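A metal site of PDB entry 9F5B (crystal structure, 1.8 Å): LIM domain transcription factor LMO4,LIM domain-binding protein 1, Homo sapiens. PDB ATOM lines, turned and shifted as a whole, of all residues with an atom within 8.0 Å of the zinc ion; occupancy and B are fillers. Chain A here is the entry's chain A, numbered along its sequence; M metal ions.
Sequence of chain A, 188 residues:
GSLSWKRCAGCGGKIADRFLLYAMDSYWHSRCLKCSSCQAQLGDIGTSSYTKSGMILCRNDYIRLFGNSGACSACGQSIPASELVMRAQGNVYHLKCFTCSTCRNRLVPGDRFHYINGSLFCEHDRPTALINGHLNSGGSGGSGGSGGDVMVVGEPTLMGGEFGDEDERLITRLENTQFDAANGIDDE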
ATOM      1  N   THR A  99      -5.787  -0.365  13.856  1.00  0.00           N
ATOM      2  CA  THR A  99      -4.372   0.063  13.798  1.00  0.00           C
ATOM      3  C   THR A  99      -4.137   1.469  14.370  1.00  0.00           C
ATOM      4  O   THR A  99      -5.070   2.253  14.441  1.00  0.00           O
ATOM      5  CB  THR A  99      -3.855  -0.013  12.355  1.00  0.00           C
ATOM      6  OG1 THR A  99      -4.638   0.866  11.530  1.00  0.00           O
ATOM      7  CG2 THR A  99      -4.109  -1.388  11.760  1.00  0.00           C
ATOM      8  N   CYS A 100      -2.893   1.757  14.755  1.00  0.00           N
ATOM      9  CA  CYS A 100      -2.501   3.083  15.221  1.00  0.00           C
ATOM     10  C   CYS A 100      -2.523   4.082  14.058  1.00  0.00           C
ATOM     11  O   CYS A 100      -1.902   3.845  13.027  1.00  0.00           O
ATOM     12  CB  CYS A 100      -1.115   3.032  15.838  1.00  0.00           C
ATOM     13  SG  CYS A 100      -0.438   4.636  16.378  1.00  0.00           S
ATOM     14  N   SER A 101      -3.198   5.213  14.262  1.00  0.00           N
ATOM     15  CA  SER A 101      -3.308   6.213  13.215  1.00  0.00           C
ATOM     16  C   SER A 101      -1.959   6.871  12.876  1.00  0.00           C
ATOM     17  O   SER A 101      -1.812   7.420  11.793  1.00  0.00           O
ATOM     18  CB  SER A 101      -4.341   7.284  13.577  1.00  0.00           C
ATOM     19  OG  SER A 101      -5.653   6.740  13.635  1.00  0.00           O
ATOM     20  N   THR A 102      -1.002   6.828  13.803  1.00  0.00           N
ATOM     21  CA  THR A 102       0.318   7.426  13.593  1.00  0.00           C
ATOM     22  C   THR A 102       1.321   6.440  12.964  1.00  0.00           C
ATOM     23  O   THR A 102       1.867   6.724  11.900  1.00  0.00           O
ATOM     24  CB  THR A 102       0.859   7.983  14.916  1.00  0.00           C
ATOM     25  OG1 THR A 102      -0.054   8.955  15.426  1.00  0.00           O
ATOM     26  CG2 THR A 102       2.222   8.623  14.716  1.00  0.00           C
ATOM     27  N   CYS A 103       1.569   5.291  13.610  1.00  0.00           N
ATOM     28  CA  CYS A 103       2.634   4.393  13.167  1.00  0.00           C
ATOM     29  C   CYS A 103       2.130   3.229  12.311  1.00  0.00           C
ATOM     30  O   CYS A 103       2.932   2.511  11.723  1.00  0.00           O
ATOM     31  CB  CYS A 103       3.423   3.842  14.363  1.00  0.00           C
ATOM     32  SG  CYS A 103       2.556   2.594  15.359  1.00  0.00           S
ATOM     33  N   ARG A 104       0.825   3.015  12.296  1.00  0.00           N
ATOM     34  CA  ARG A 104       0.080   2.007  11.546  1.00  0.00           C
ATOM     35  C   ARG A 104       0.177   0.593  12.119  1.00  0.00           C
ATOM     36  O   ARG A 104      -0.375  -0.340  11.517  1.00  0.00           O
ATOM     37  CB  ARG A 104       0.388   1.987  10.040  1.00  0.00           C
ATOM     38  CG  ARG A 104      -0.103   3.271   9.381  1.00  0.00           C
ATOM     39  CD  ARG A 104       0.379   3.370   7.952  1.00  0.00           C
ATOM     40  NE  ARG A 104      -0.315   4.561   7.470  1.00  0.00           N
ATOM     41  CZ  ARG A 104      -0.116   5.154   6.304  1.00  0.00           C
ATOM     42  NH1 ARG A 104       0.808   4.695   5.469  1.00  0.00           N
ATOM     43  NH2 ARG A 104      -0.827   6.210   5.965  1.00  0.00           N
ATOM     44  N   ASN A 105       0.837   0.414  13.276  1.00  0.00           N
ATOM     45  CA  ASN A 105       0.873  -0.894  13.918  1.00  0.00           C
ATOM     46  C   ASN A 105      -0.533  -1.411  14.222  1.00  0.00           C
ATOM     47  O   ASN A 105      -1.402  -0.667  14.695  1.00  0.00           O
ATOM     48  CB  ASN A 105       1.645  -0.800  15.234  1.00  0.00           C
ATOM     49  CG  ASN A 105       3.121  -1.021  15.095  1.00  0.00           C
ATOM     50  OD1 ASN A 105       3.699  -0.843  14.003  1.00  0.00           O
ATOM     51  ND2 ASN A 105       3.762  -1.353  16.204  1.00  0.00           N
ATOM     52  N   ARG A 106      -0.748  -2.698  13.947  1.00  0.00           N
ATOM     53  CA  ARG A 106      -1.967  -3.372  14.373  1.00  0.00           C
ATOM     54  C   ARG A 106      -1.963  -3.561  15.882  1.00  0.00           C
ATOM     55  O   ARG A 106      -1.010  -4.092  16.461  1.00  0.00           O
ATOM     56  CB  ARG A 106      -2.088  -4.707  13.620  1.00  0.00           C
ATOM     57  CG  ARG A 106      -3.415  -5.435  13.756  1.00  0.00           C
ATOM     58  CD  ARG A 106      -3.375  -6.749  12.995  1.00  0.00           C
ATOM     59  NE  ARG A 106      -2.826  -6.543  11.653  1.00  0.00           N
ATOM     60  CZ  ARG A 106      -2.102  -7.430  10.952  1.00  0.00           C
ATOM     61  NH1 ARG A 106      -1.904  -8.650  11.406  1.00  0.00           N
ATOM     62  NH2 ARG A 106      -1.570  -7.087   9.789  1.00  0.00           N
ATOM     63  N   LEU A 107      -3.056  -3.144  16.515  1.00  0.00           N
ATOM     64  CA  LEU A 107      -3.229  -3.251  17.967  1.00  0.00           C
ATOM     65  C   LEU A 107      -3.802  -4.614  18.350  1.00  0.00           C
ATOM     66  O   LEU A 107      -4.689  -5.137  17.662  1.00  0.00           O
ATOM     67  CB  LEU A 107      -4.177  -2.145  18.449  1.00  0.00           C
ATOM     68  CG  LEU A 107      -3.784  -0.693  18.153  1.00  0.00           C
ATOM     69  CD1 LEU A 107      -4.997   0.165  18.424  1.00  0.00           C
ATOM     70  CD2 LEU A 107      -2.560  -0.233  18.952  1.00  0.00           C
ATOM     71  N   ARG A 112      -1.932  -1.153  25.358  1.00  0.00           N
ATOM     72  CA  ARG A 112      -2.464   0.139  25.774  1.00  0.00           C
ATOM     73  C   ARG A 112      -2.661   1.031  24.547  1.00  0.00           C
ATOM     74  O   ARG A 112      -1.849   1.017  23.629  1.00  0.00           O
ATOM     75  CB  ARG A 112      -1.510   0.791  26.782  1.00  0.00           C
ATOM     76  CG  ARG A 112      -1.552   0.178  28.186  1.00  0.00           C
ATOM     77  CD  ARG A 112      -0.407   0.726  29.030  1.00  0.00           C
ATOM     78  NE  ARG A 112      -0.725   1.045  30.425  1.00  0.00           N
ATOM     79  CZ  ARG A 112      -0.668   0.206  31.442  1.00  0.00           C
ATOM     80  NH1 ARG A 112      -0.398  -1.084  31.258  1.00  0.00           N
ATOM     81  NH2 ARG A 112      -0.845   0.650  32.670  1.00  0.00           N
ATOM     82  N   LEU A 120      -7.388   5.949  16.445  1.00  0.00           N
ATOM     83  CA  LEU A 120      -6.696   5.082  17.399  1.00  0.00           C
ATOM     84  C   LEU A 120      -5.199   5.393  17.413  1.00  0.00           C
ATOM     85  O   LEU A 120      -4.599   5.606  16.370  1.00  0.00           O
ATOM     86  CB  LEU A 120      -6.923   3.603  17.056  1.00  0.00           C
ATOM     87  CG  LEU A 120      -8.364   3.068  17.057  1.00  0.00           C
ATOM     88  CD1 LEU A 120      -8.483   1.823  16.182  1.00  0.00           C
ATOM     89  CD2 LEU A 120      -8.798   2.756  18.483  1.00  0.00           C
ATOM     90  N   PHE A 121      -4.573   5.334  18.601  1.00  0.00           N
ATOM     91  CA  PHE A 121      -3.150   5.558  18.739  1.00  0.00           C
ATOM     92  C   PHE A 121      -2.551   4.550  19.722  1.00  0.00           C
ATOM     93  O   PHE A 121      -3.138   4.302  20.765  1.00  0.00           O
ATOM     94  CB  PHE A 121      -2.850   6.966  19.259  1.00  0.00           C
ATOM     95  CG  PHE A 121      -3.346   8.078  18.372  1.00  0.00           C
ATOM     96  CD1 PHE A 121      -2.608   8.512  17.299  1.00  0.00           C
ATOM     97  CD2 PHE A 121      -4.562   8.684  18.642  1.00  0.00           C
ATOM     98  CE1 PHE A 121      -3.079   9.548  16.495  1.00  0.00           C
ATOM     99  CE2 PHE A 121      -5.033   9.717  17.848  1.00  0.00           C
ATOM    100  CZ  PHE A 121      -4.295  10.154  16.766  1.00  0.00           C
ATOM    101  N   CYS A 122      -1.411   3.944  19.370  1.00  0.00           N
ATOM    102  CA  CYS A 122      -0.761   3.026  20.292  1.00  0.00           C
ATOM    103  C   CYS A 122      -0.112   3.784  21.446  1.00  0.00           C
ATOM    104  O   CYS A 122      -0.004   5.015  21.431  1.00  0.00           O
ATOM    105  CB  CYS A 122       0.312   2.196  19.587  1.00  0.00           C
ATOM    106  SG  CYS A 122       1.862   3.078  19.279  1.00  0.00           S
ATOM    107  N   GLU A 123       0.333   3.027  22.444  1.00  0.00           N
ATOM    108  CA  GLU A 123       0.904   3.586  23.663  1.00  0.00           C
ATOM    109  C   GLU A 123       2.077   4.541  23.381  1.00  0.00           C
ATOM    110  O   GLU A 123       2.262   5.519  24.095  1.00  0.00           O
ATOM    111  CB  GLU A 123       1.361   2.447  24.575  1.00  0.00           C
ATOM    112  CG  GLU A 123       1.743   2.916  25.972  1.00  0.00           C
ATOM    113  CD  GLU A 123       2.155   1.745  26.836  1.00  0.00           C
ATOM    114  OE1 GLU A 123       2.075   0.572  26.401  1.00  0.00           O
ATOM    115  OE2 GLU A 123       2.557   1.974  27.998  1.00  0.00           O
ATOM    116  N   HIS A 124       2.860   4.271  22.348  1.00  0.00           N
ATOM    117  CA  HIS A 124       4.078   5.026  22.066  1.00  0.00           C
ATOM    118  C   HIS A 124       3.846   6.155  21.074  1.00  0.00           C
ATOM    119  O   HIS A 124       4.806   6.831  20.707  1.00  0.00           O
ATOM    120  CB  HIS A 124       5.151   4.087  21.499  1.00  0.00           C
ATOM    121  CG  HIS A 124       5.368   2.886  22.360  1.00  0.00           C
ATOM    122  ND1 HIS A 124       5.904   2.977  23.628  1.00  0.00           N
ATOM    123  CD2 HIS A 124       5.038   1.582  22.197  1.00  0.00           C
ATOM    124  CE1 HIS A 124       5.916   1.793  24.199  1.00  0.00           C
ATOM    125  NE2 HIS A 124       5.400   0.927  23.355  1.00  0.00           N
ATOM    126  N   ASP A 125       2.603   6.369  20.660  1.00  0.00           N
ATOM    127  CA  ASP A 125       2.198   7.489  19.825  1.00  0.00           C
ATOM    128  C   ASP A 125       1.077   8.261  20.496  1.00  0.00           C
ATOM    129  O   ASP A 125       0.131   8.704  19.833  1.00  0.00           O
ATOM    130  CB  ASP A 125       1.772   7.025  18.440  1.00  0.00           C
ATOM    131  CG  ASP A 125       2.947   6.613  17.580  1.00  0.00           C
ATOM    132  OD1 ASP A 125       3.947   7.358  17.548  1.00  0.00           O
ATOM    133  OD2 ASP A 125       2.865   5.561  16.958  1.00  0.00           O
ATOM    134  N   ARG A 126       1.179   8.422  21.822  1.00  0.00           N
ATOM    135  CA  ARG A 126       0.246   9.272  22.539  1.00  0.00           C
ATOM    136  C   ARG A 126       0.188  10.635  21.839  1.00  0.00           C
ATOM    137  O   ARG A 126       1.206  11.321  21.730  1.00  0.00           O
ATOM    138  CB  ARG A 126       0.723   9.406  23.974  1.00  0.00           C
ATOM    139  CG  ARG A 126      -0.177  10.254  24.865  1.00  0.00           C
ATOM    140  CD  ARG A 126       0.497  10.465  26.212  1.00  0.00           C
ATOM    141  NE  ARG A 126      -0.432  11.082  27.149  1.00  0.00           N
ATOM    142  CZ  ARG A 126      -0.672  12.374  27.229  1.00  0.00           C
ATOM    143  NH1 ARG A 126      -0.055  13.230  26.429  1.00  0.00           N
ATOM    144  NH2 ARG A 126      -1.545  12.820  28.122  1.00  0.00           N
HETATM  145 ZN    ZN M   1       1.737   3.793  17.099  1.00  0.00          ZN
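The side-chain sulfur (SG) of Cys 100 lies close to the backbone NH (N) of Thr 102 (3.4 Å). The backbone carbonyl oxygen (O) of Asn 105 lies within hydrogen-bond range of the backbone NH (N) of Cys 100, 2.8 Å away. The backbone NH (N) of Asn 105 lies close to the side-chain sulfur (SG) of Cys 103. SG of Cys 122 lies close to N of His 124 (3.4 Å).
The zinc ion is bound by OD2 of Asp 125 (2.1 Å), SG of Cys 103 (2.3 Å), SG of Cys 122 (2.3 Å) and SG of Cys 100 (2.4 Å).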
